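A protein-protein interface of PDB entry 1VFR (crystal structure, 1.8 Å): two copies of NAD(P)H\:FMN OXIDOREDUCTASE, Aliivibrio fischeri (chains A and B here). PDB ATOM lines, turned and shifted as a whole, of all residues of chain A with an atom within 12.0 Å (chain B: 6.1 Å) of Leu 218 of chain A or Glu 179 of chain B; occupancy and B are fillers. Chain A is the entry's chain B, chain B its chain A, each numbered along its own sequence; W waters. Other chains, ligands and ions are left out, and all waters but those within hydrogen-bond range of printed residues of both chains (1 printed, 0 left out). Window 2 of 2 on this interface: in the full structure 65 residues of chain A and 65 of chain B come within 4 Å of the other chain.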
ATOM      1  N   LYS A 209     -29.815  17.483  17.252  1.00  0.00           N
ATOM      2  CA  LYS A 209     -29.337  17.395  18.623  1.00  0.00           C
ATOM      3  C   LYS A 209     -27.990  16.696  18.678  1.00  0.00           C
ATOM      4  O   LYS A 209     -27.646  15.892  17.805  1.00  0.00           O
ATOM      5  CB  LYS A 209     -30.311  16.597  19.487  1.00  0.00           C
ATOM      6  CG  LYS A 209     -31.601  17.296  19.838  1.00  0.00           C
ATOM      7  CD  LYS A 209     -32.544  16.264  20.422  1.00  0.00           C
ATOM      8  CE  LYS A 209     -33.840  16.863  20.847  1.00  0.00           C
ATOM      9  NZ  LYS A 209     -34.770  15.793  21.316  1.00  0.00           N
ATOM     10  N   PHE A 211     -25.095  14.191  19.527  1.00  0.00           N
ATOM     11  CA  PHE A 211     -25.049  12.747  19.548  1.00  0.00           C
ATOM     12  C   PHE A 211     -25.373  12.184  20.938  1.00  0.00           C
ATOM     13  O   PHE A 211     -26.155  11.248  21.042  1.00  0.00           O
ATOM     14  CB  PHE A 211     -23.657  12.288  19.097  1.00  0.00           C
ATOM     15  CG  PHE A 211     -23.520  10.800  18.932  1.00  0.00           C
ATOM     16  CD1 PHE A 211     -23.391   9.971  20.036  1.00  0.00           C
ATOM     17  CD2 PHE A 211     -23.462  10.235  17.662  1.00  0.00           C
ATOM     18  CE1 PHE A 211     -23.201   8.601  19.885  1.00  0.00           C
ATOM     19  CE2 PHE A 211     -23.273   8.868  17.503  1.00  0.00           C
ATOM     20  CZ  PHE A 211     -23.140   8.054  18.625  1.00  0.00           C
ATOM     21  N   GLU A 212     -24.804  12.746  22.007  1.00  0.00           N
ATOM     22  CA  GLU A 212     -25.087  12.231  23.365  1.00  0.00           C
ATOM     23  C   GLU A 212     -26.484  12.527  23.888  1.00  0.00           C
ATOM     24  O   GLU A 212     -26.922  11.931  24.883  1.00  0.00           O
ATOM     25  CB  GLU A 212     -24.055  12.688  24.407  1.00  0.00           C
ATOM     26  CG  GLU A 212     -23.713  14.162  24.353  1.00  0.00           C
ATOM     27  CD  GLU A 212     -22.788  14.482  23.183  1.00  0.00           C
ATOM     28  OE1 GLU A 212     -21.979  13.598  22.793  1.00  0.00           O
ATOM     29  OE2 GLU A 212     -22.885  15.607  22.643  1.00  0.00           O
ATOM     30  N   ASP A 213     -27.170  13.462  23.246  1.00  0.00           N
ATOM     31  CA  ASP A 213     -28.521  13.779  23.649  1.00  0.00           C
ATOM     32  C   ASP A 213     -29.547  12.799  23.078  1.00  0.00           C
ATOM     33  O   ASP A 213     -30.618  12.609  23.663  1.00  0.00           O
ATOM     34  CB  ASP A 213     -28.882  15.200  23.237  1.00  0.00           C
ATOM     35  CG  ASP A 213     -28.162  16.254  24.065  1.00  0.00           C
ATOM     36  OD1 ASP A 213     -27.494  15.912  25.064  1.00  0.00           O
ATOM     37  OD2 ASP A 213     -28.271  17.440  23.719  1.00  0.00           O
ATOM     38  N   VAL A 214     -29.218  12.151  21.959  1.00  0.00           N
ATOM     39  CA  VAL A 214     -30.155  11.212  21.329  1.00  0.00           C
ATOM     40  C   VAL A 214     -29.729   9.749  21.300  1.00  0.00           C
ATOM     41  O   VAL A 214     -30.558   8.873  21.068  1.00  0.00           O
ATOM     42  CB  VAL A 214     -30.518  11.643  19.875  1.00  0.00           C
ATOM     43  CG1 VAL A 214     -31.392  12.861  19.902  1.00  0.00           C
ATOM     44  CG2 VAL A 214     -29.267  11.914  19.048  1.00  0.00           C
ATOM     45  N   ILE A 215     -28.442   9.479  21.530  1.00  0.00           N
ATOM     46  CA  ILE A 215     -27.935   8.108  21.487  1.00  0.00           C
ATOM     47  C   ILE A 215     -27.271   7.705  22.806  1.00  0.00           C
ATOM     48  O   ILE A 215     -26.486   8.467  23.368  1.00  0.00           O
ATOM     49  CB  ILE A 215     -26.914   7.924  20.278  1.00  0.00           C
ATOM     50  CG1 ILE A 215     -27.652   8.095  18.939  1.00  0.00           C
ATOM     51  CG2 ILE A 215     -26.244   6.532  20.317  1.00  0.00           C
ATOM     52  CD1 ILE A 215     -26.774   8.507  17.810  1.00  0.00           C
ATOM     53  N   THR A 216     -27.611   6.515  23.293  1.00  0.00           N
ATOM     54  CA  THR A 216     -27.032   5.986  24.508  1.00  0.00           C
ATOM     55  C   THR A 216     -26.507   4.617  24.175  1.00  0.00           C
ATOM     56  O   THR A 216     -27.233   3.809  23.624  1.00  0.00           O
ATOM     57  CB  THR A 216     -28.088   5.816  25.610  1.00  0.00           C
ATOM     58  OG1 THR A 216     -28.613   7.094  25.967  1.00  0.00           O
ATOM     59  CG2 THR A 216     -27.470   5.142  26.835  1.00  0.00           C
ATOM     60  N   ILE A 217     -25.250   4.343  24.521  1.00  0.00           N
ATOM     61  CA  ILE A 217     -24.661   3.034  24.257  1.00  0.00           C
ATOM     62  C   ILE A 217     -24.467   2.307  25.595  1.00  0.00           C
ATOM     63  O   ILE A 217     -23.835   2.817  26.510  1.00  0.00           O
ATOM     64  CB  ILE A 217     -23.343   3.157  23.433  1.00  0.00           C
ATOM     65  CG1 ILE A 217     -23.635   3.946  22.143  1.00  0.00           C
ATOM     66  CG2 ILE A 217     -22.776   1.766  23.111  1.00  0.00           C
ATOM     67  CD1 ILE A 217     -22.453   4.232  21.293  1.00  0.00           C
ATOM     68  N   LEU A 218     -25.089   1.144  25.712  1.00  0.00           N
ATOM     69  CA  LEU A 218     -25.034   0.341  26.916  1.00  0.00           C
ATOM     70  C   LEU A 218     -24.279  -0.959  26.746  1.00  0.00           C
ATOM     71  O   LEU A 218     -23.906  -1.536  27.790  1.00  0.00           O
ATOM     72  CB  LEU A 218     -26.445   0.013  27.377  1.00  0.00           C
ATOM     73  CG  LEU A 218     -27.369   1.192  27.651  1.00  0.00           C
ATOM     74  CD1 LEU A 218     -28.738   0.648  28.043  1.00  0.00           C
ATOM     75  CD2 LEU A 218     -26.816   2.077  28.764  1.00  0.00           C
ATOM     76  OXT LEU A 218     -24.109  -1.421  25.601  1.00  0.00           O
ATOM     77  N   LYS B  49     -35.065   8.786  21.238  1.00  0.00           N
ATOM     78  CA  LYS B  49     -33.831   8.401  21.885  1.00  0.00           C
ATOM     79  C   LYS B  49     -33.526   7.010  21.311  1.00  0.00           C
ATOM     80  O   LYS B  49     -34.430   6.180  21.197  1.00  0.00           O
ATOM     81  CB  LYS B  49     -34.059   8.338  23.398  1.00  0.00           C
ATOM     82  CG  LYS B  49     -32.831   8.168  24.234  1.00  0.00           C
ATOM     83  CD  LYS B  49     -33.142   8.544  25.680  1.00  0.00           C
ATOM     84  CE  LYS B  49     -31.999   8.139  26.593  1.00  0.00           C
ATOM     85  NZ  LYS B  49     -32.230   8.491  28.018  1.00  0.00           N
ATOM     86  N   ILE B  51     -31.375   3.784  21.932  1.00  0.00           N
ATOM     87  CA  ILE B  51     -30.579   3.080  22.918  1.00  0.00           C
ATOM     88  C   ILE B  51     -29.935   1.874  22.276  1.00  0.00           C
ATOM     89  O   ILE B  51     -30.620   0.975  21.813  1.00  0.00           O
ATOM     90  CB  ILE B  51     -31.461   2.653  24.092  1.00  0.00           C
ATOM     91  CG1 ILE B  51     -32.066   3.907  24.728  1.00  0.00           C
ATOM     92  CG2 ILE B  51     -30.662   1.824  25.103  1.00  0.00           C
ATOM     93  CD1 ILE B  51     -33.270   3.607  25.565  1.00  0.00           C
ATOM     94  N   VAL B  52     -28.608   1.877  22.246  1.00  0.00           N
ATOM     95  CA  VAL B  52     -27.836   0.795  21.646  1.00  0.00           C
ATOM     96  C   VAL B  52     -27.390  -0.222  22.697  1.00  0.00           C
ATOM     97  O   VAL B  52     -26.700   0.110  23.652  1.00  0.00           O
ATOM     98  CB  VAL B  52     -26.602   1.349  20.880  1.00  0.00           C
ATOM     99  CG1 VAL B  52     -25.908   0.219  20.077  1.00  0.00           C
ATOM    100  CG2 VAL B  52     -27.027   2.509  19.959  1.00  0.00           C
ATOM    101  N   ILE B  53     -27.810  -1.459  22.512  1.00  0.00           N
ATOM    102  CA  ILE B  53     -27.489  -2.559  23.391  1.00  0.00           C
ATOM    103  C   ILE B  53     -26.253  -3.196  22.772  1.00  0.00           C
ATOM    104  O   ILE B  53     -26.342  -3.935  21.787  1.00  0.00           O
ATOM    105  CB  ILE B  53     -28.663  -3.567  23.410  1.00  0.00           C
ATOM    106  CG1 ILE B  53     -29.976  -2.863  23.782  1.00  0.00           C
ATOM    107  CG2 ILE B  53     -28.355  -4.748  24.290  1.00  0.00           C
ATOM    108  CD1 ILE B  53     -29.948  -2.153  25.083  1.00  0.00           C
ATOM    109  N   GLU B  54     -25.097  -2.928  23.358  1.00  0.00           N
ATOM    110  CA  GLU B  54     -23.841  -3.453  22.835  1.00  0.00           C
ATOM    111  C   GLU B  54     -23.110  -4.442  23.731  1.00  0.00           C
ATOM    112  O   GLU B  54     -22.732  -5.518  23.283  1.00  0.00           O
ATOM    113  CB  GLU B  54     -22.916  -2.288  22.494  1.00  0.00           C
ATOM    114  CG  GLU B  54     -21.541  -2.707  22.008  1.00  0.00           C
ATOM    115  CD  GLU B  54     -20.740  -1.537  21.515  1.00  0.00           C
ATOM    116  OE1 GLU B  54     -20.308  -0.715  22.346  1.00  0.00           O
ATOM    117  OE2 GLU B  54     -20.543  -1.420  20.292  1.00  0.00           O
ATOM    118  N   SER B  55     -22.948  -4.093  25.008  1.00  0.00           N
ATOM    119  CA  SER B  55     -22.231  -4.945  25.953  1.00  0.00           C
ATOM    120  C   SER B  55     -22.957  -6.231  26.302  1.00  0.00           C
ATOM    121  O   SER B  55     -24.172  -6.339  26.143  1.00  0.00           O
ATOM    122  CB  SER B  55     -21.953  -4.155  27.234  1.00  0.00           C
ATOM    123  OG  SER B  55     -23.129  -4.020  28.007  1.00  0.00           O
ATOM    124  N   ASP B  56     -22.214  -7.210  26.797  1.00  0.00           N
ATOM    125  CA  ASP B  56     -22.821  -8.464  27.204  1.00  0.00           C
ATOM    126  C   ASP B  56     -23.819  -8.212  28.338  1.00  0.00           C
ATOM    127  O   ASP B  56     -24.852  -8.868  28.411  1.00  0.00           O
ATOM    128  CB  ASP B  56     -21.757  -9.454  27.679  1.00  0.00           C
ATOM    129  CG  ASP B  56     -21.080 -10.197  26.535  1.00  0.00           C
ATOM    130  OD1 ASP B  56     -21.247  -9.812  25.350  1.00  0.00           O
ATOM    131  OD2 ASP B  56     -20.370 -11.188  26.823  1.00  0.00           O
ATOM    132  N   ALA B  57     -23.495  -7.270  29.225  1.00  0.00           N
ATOM    133  CA  ALA B  57     -24.363  -6.938  30.352  1.00  0.00           C
ATOM    134  C   ALA B  57     -25.681  -6.388  29.819  1.00  0.00           C
ATOM    135  O   ALA B  57     -26.747  -6.800  30.258  1.00  0.00           O
ATOM    136  CB  ALA B  57     -23.686  -5.922  31.269  1.00  0.00           C
ATOM    137  N   ALA B  58     -25.597  -5.493  28.837  1.00  0.00           N
ATOM    138  CA  ALA B  58     -26.789  -4.910  28.237  1.00  0.00           C
ATOM    139  C   ALA B  58     -27.570  -5.970  27.459  1.00  0.00           C
ATOM    140  O   ALA B  58     -28.790  -5.952  27.443  1.00  0.00           O
ATOM    141  CB  ALA B  58     -26.426  -3.750  27.343  1.00  0.00           C
ATOM    142  N   ARG B  61     -29.789  -7.930  29.881  1.00  0.00           N
ATOM    143  CA  ARG B  61     -30.965  -7.161  30.287  1.00  0.00           C
ATOM    144  C   ARG B  61     -32.018  -7.207  29.201  1.00  0.00           C
ATOM    145  O   ARG B  61     -33.193  -7.362  29.483  1.00  0.00           O
ATOM    146  CB  ARG B  61     -30.579  -5.706  30.552  1.00  0.00           C
ATOM    147  CG  ARG B  61     -29.701  -5.524  31.807  1.00  0.00           C
ATOM    148  CD  ARG B  61     -28.996  -4.172  31.817  1.00  0.00           C
ATOM    149  NE  ARG B  61     -29.918  -3.073  32.057  1.00  0.00           N
ATOM    150  CZ  ARG B  61     -29.610  -1.788  31.903  1.00  0.00           C
ATOM    151  NH1 ARG B  61     -28.410  -1.418  31.496  1.00  0.00           N
ATOM    152  NH2 ARG B  61     -30.481  -0.857  32.233  1.00  0.00           N
ATOM    153  N   ILE B 175     -36.711  -2.706  33.150  1.00  0.00           N
ATOM    154  CA  ILE B 175     -35.333  -3.102  32.956  1.00  0.00           C
ATOM    155  C   ILE B 175     -34.414  -1.932  32.567  1.00  0.00           C
ATOM    156  O   ILE B 175     -33.283  -1.845  33.052  1.00  0.00           O
ATOM    157  CB  ILE B 175     -35.270  -4.242  31.950  1.00  0.00           C
ATOM    158  CG1 ILE B 175     -36.043  -5.429  32.508  1.00  0.00           C
ATOM    159  CG2 ILE B 175     -33.821  -4.611  31.636  1.00  0.00           C
ATOM    160  CD1 ILE B 175     -36.046  -6.613  31.621  1.00  0.00           C
ATOM    161  N   PHE B 176     -34.903  -1.030  31.714  1.00  0.00           N
ATOM    162  CA  PHE B 176     -34.144   0.144  31.288  1.00  0.00           C
ATOM    163  C   PHE B 176     -34.799   1.374  31.880  1.00  0.00           C
ATOM    164  O   PHE B 176     -35.012   2.379  31.202  1.00  0.00           O
ATOM    165  CB  PHE B 176     -34.091   0.245  29.763  1.00  0.00           C
ATOM    166  CG  PHE B 176     -33.358  -0.881  29.123  1.00  0.00           C
ATOM    167  CD1 PHE B 176     -31.971  -0.909  29.118  1.00  0.00           C
ATOM    168  CD2 PHE B 176     -34.051  -1.966  28.600  1.00  0.00           C
ATOM    169  CE1 PHE B 176     -31.287  -2.005  28.613  1.00  0.00           C
ATOM    170  CE2 PHE B 176     -33.368  -3.072  28.086  1.00  0.00           C
ATOM    171  CZ  PHE B 176     -31.981  -3.090  28.096  1.00  0.00           C
ATOM    172  N   ALA B 177     -35.053   1.290  33.187  1.00  0.00           N
ATOM    173  CA  ALA B 177     -35.715   2.330  33.968  1.00  0.00           C
ATOM    174  C   ALA B 177     -35.216   3.729  33.772  1.00  0.00           C
ATOM    175  O   ALA B 177     -35.990   4.624  33.453  1.00  0.00           O
ATOM    176  CB  ALA B 177     -35.672   1.970  35.465  1.00  0.00           C
ATOM    177  N   ASP B 178     -33.926   3.935  33.981  1.00  0.00           N
ATOM    178  CA  ASP B 178     -33.395   5.266  33.842  1.00  0.00           C
ATOM    179  C   ASP B 178     -33.258   5.753  32.398  1.00  0.00           C
ATOM    180  O   ASP B 178     -33.517   6.922  32.106  1.00  0.00           O
ATOM    181  CB  ASP B 178     -32.069   5.375  34.574  1.00  0.00           C
ATOM    182  CG  ASP B 178     -31.842   6.747  35.128  1.00  0.00           C
ATOM    183  OD1 ASP B 178     -32.749   7.257  35.822  1.00  0.00           O
ATOM    184  OD2 ASP B 178     -30.776   7.330  34.855  1.00  0.00           O
ATOM    185  N   GLU B 179     -32.914   4.847  31.497  1.00  0.00           N
ATOM    186  CA  GLU B 179     -32.714   5.208  30.090  1.00  0.00           C
ATOM    187  C   GLU B 179     -34.016   5.574  29.383  1.00  0.00           C
ATOM    188  O   GLU B 179     -34.038   6.467  28.544  1.00  0.00           O
ATOM    189  CB  GLU B 179     -31.995   4.072  29.344  1.00  0.00           C
ATOM    190  CG  GLU B 179     -30.662   3.674  29.956  1.00  0.00           C
ATOM    191  CD  GLU B 179     -30.760   2.551  30.997  1.00  0.00           C
ATOM    192  OE1 GLU B 179     -31.842   2.343  31.599  1.00  0.00           O
ATOM    193  OE2 GLU B 179     -29.749   1.845  31.203  1.00  0.00           O
ATOM    194  N   LEU B 180     -35.099   4.902  29.751  1.00  0.00           N
ATOM    195  CA  LEU B 180     -36.403   5.141  29.135  1.00  0.00           C
ATOM    196  C   LEU B 180     -37.334   6.062  29.924  1.00  0.00           C
ATOM    197  O   LEU B 180     -38.514   6.172  29.602  1.00  0.00           O
ATOM    198  CB  LEU B 180     -37.106   3.808  28.869  1.00  0.00           C
ATOM    199  CG  LEU B 180     -36.529   2.938  27.745  1.00  0.00           C
ATOM    200  CD1 LEU B 180     -37.230   1.610  27.688  1.00  0.00           C
ATOM    201  CD2 LEU B 180     -36.675   3.651  26.429  1.00  0.00           C
ATOM    202  N   LYS B 181     -36.828   6.704  30.974  1.00  0.00           N
ATOM    203  CA  LYS B 181     -37.667   7.595  31.761  1.00  0.00           C
ATOM    204  C   LYS B 181     -38.166   8.749  30.900  1.00  0.00           C
ATOM    205  O   LYS B 181     -37.369   9.505  30.347  1.00  0.00           O
ATOM    206  CB  LYS B 181     -36.916   8.114  33.009  1.00  0.00           C
ATOM    207  CG  LYS B 181     -37.310   7.372  34.306  1.00  0.00           C
ATOM    208  CD  LYS B 181     -36.193   7.379  35.377  1.00  0.00           C
ATOM    209  CE  LYS B 181     -36.405   6.287  36.448  1.00  0.00           C
ATOM    210  NZ  LYS B 181     -35.160   6.021  37.252  1.00  0.00           N
ATOM    211  N   TYR B 183     -40.054   8.206  28.238  1.00  0.00           N
ATOM    212  CA  TYR B 183     -40.199   7.644  26.899  1.00  0.00           C
ATOM    213  C   TYR B 183     -40.903   6.307  26.989  1.00  0.00           C
ATOM    214  O   TYR B 183     -41.118   5.768  28.075  1.00  0.00           O
ATOM    215  CB  TYR B 183     -38.798   7.374  26.294  1.00  0.00           C
ATOM    216  CG  TYR B 183     -38.012   8.601  25.943  1.00  0.00           C
ATOM    217  CD1 TYR B 183     -37.374   9.349  26.925  1.00  0.00           C
ATOM    218  CD2 TYR B 183     -37.965   9.061  24.638  1.00  0.00           C
ATOM    219  CE1 TYR B 183     -36.722  10.526  26.617  1.00  0.00           C
ATOM    220  CE2 TYR B 183     -37.317  10.239  24.318  1.00  0.00           C
ATOM    221  CZ  TYR B 183     -36.702  10.972  25.316  1.00  0.00           C
ATOM    222  OH  TYR B 183     -36.121  12.181  25.024  1.00  0.00           O
HETATM  223  O   HOH W   1     -25.564  -2.294  30.598  1.00  0.00           O
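Leu 218 of chain A touches eight residues of chain B. Lys 49 of chain B touches just these residues of chain A: Val 214 (3.4 Å) and Thr 216 (3.6 Å). Of chain A, only Leu 218 comes within 4 Å of Ile 53 of chain B. Printed residues of chain A within 4 Å of Glu 54 of chain B: Ile 217 (3.6 Å) and Leu 218 (2.9 Å). Ala 58 of chain B touches one residue of chain A. Of chain A, only Leu 218 (3.7 Å) comes within 4 Å of Phe 176 of chain B. No residue of chain A comes within 4 Å of Ala 177 of chain B. No residue of chain A comes within 4 Å of Asp 178 of chain B. No residue of chain A comes within 4 Å of Leu 180 of chain B. No residue of chain A comes within 4 Å of Lys 181 of chain B. No residue of chain A comes within 4 Å of Tyr 183 of chain B. Printed residues of chain B within 4 Å of Val 214 of chain A: Lys 49 (3.4 Å). Printed residues of chain B within 4 Å of Ile 217 of chain A: Val 52 (3.6 Å) and Glu 54 (3.6 Å). Asp 213 of chain A touches none of the printed residues of chain B. Phe 211 of chain A touches none of the printed residues of chain B. The nearest residue of chain A that does not touch Glu 179 of chain B is Thr 216 of chain A (4.7 Å).
Val 214 of chain A touches Lys 49 of chain B. Thr 216 of chain A touches Lys 49 of chain B (OG1 to CE, 3.6 Å). CA of Ile 51 of chain B touches O of Thr 216 of chain A, 3.5 Å away. CA of Ile 217 of chain A touches O of Val 52 of chain B, 3.6 Å away. Ile 217 of chain A touches Glu 54 of chain B (CG2 to OE1, 3.6 Å). Leu 218 of chain A touches Ile 51 of chain B (CD1 to CG2, 3.7 Å). Leu 218 of chain A touches Ile 53 of chain B. O of Leu 218 of chain A touches CB of Ala 58 of chain B, 3.4 Å away. Phe 176 of chain B touches Leu 218 of chain A. CD1 of Leu 218 of chain A touches OE2 of Glu 179 of chain B, 3.5 Å away.
The backbone NH (N) of Ala 57 of chain B sits close to the side-chain hydroxyl (OG) of Ser 55 of chain B, 3.5 Å away. The backbone carbonyl oxygen (O) of Glu 179 of chain B sits at hydrogen-bond distance from the side-chain amino group (NZ) of Lys 49 of chain B, 2.8 Å away. The guanidinium group (NH2) of Arg 61 of chain B is in salt-bridge range of the side-chain carboxylate (OE2) of Glu 179 of chain B, 3.0 Å away. The backbone NH (N) of Ala 58 of chain B lies within hydrogen-bond range of the side-chain hydroxyl (OG) of Ser 55 of chain B, at 3.0 Å.
The chain-end carboxylate (OXT) of Leu 218 of chain A is in hydrogen-bond range of the backbone NH (N) of Glu 54 of chain B, at 2.9 Å. N of Val 52 of chain B lies within hydrogen-bond range of O of Thr 216 of chain A (2.7 Å). O of Leu 218 of chain A lies within hydrogen-bond range of OG of Ser 55 of chain B. The backbone carbonyl oxygen (O) of Val 52 of chain B sits at hydrogen-bond distance from the backbone NH (N) of Leu 218 of chain A (2.8 Å).
Hydrophobic or aromatic side chains of chain A within 4 Å of the printed part of chain B: Ile 217 and Leu 218. Hydrophobic or aromatic side chains of chain B within 4 Å of the printed part of chain A: Ile 51, Val 52, Ala 58 and Phe 176. Along chain B the printed residues that touch a printed residue of chain A span positions 49 to 179.
Water W1 bridges NH1 of Arg 61 of chain B and O of Leu 218 of chain A.
No position is printed for both chains. Of the 14 pairs that touch across the chains among the printed residues, none has its exchanged pair printed and touching as well.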
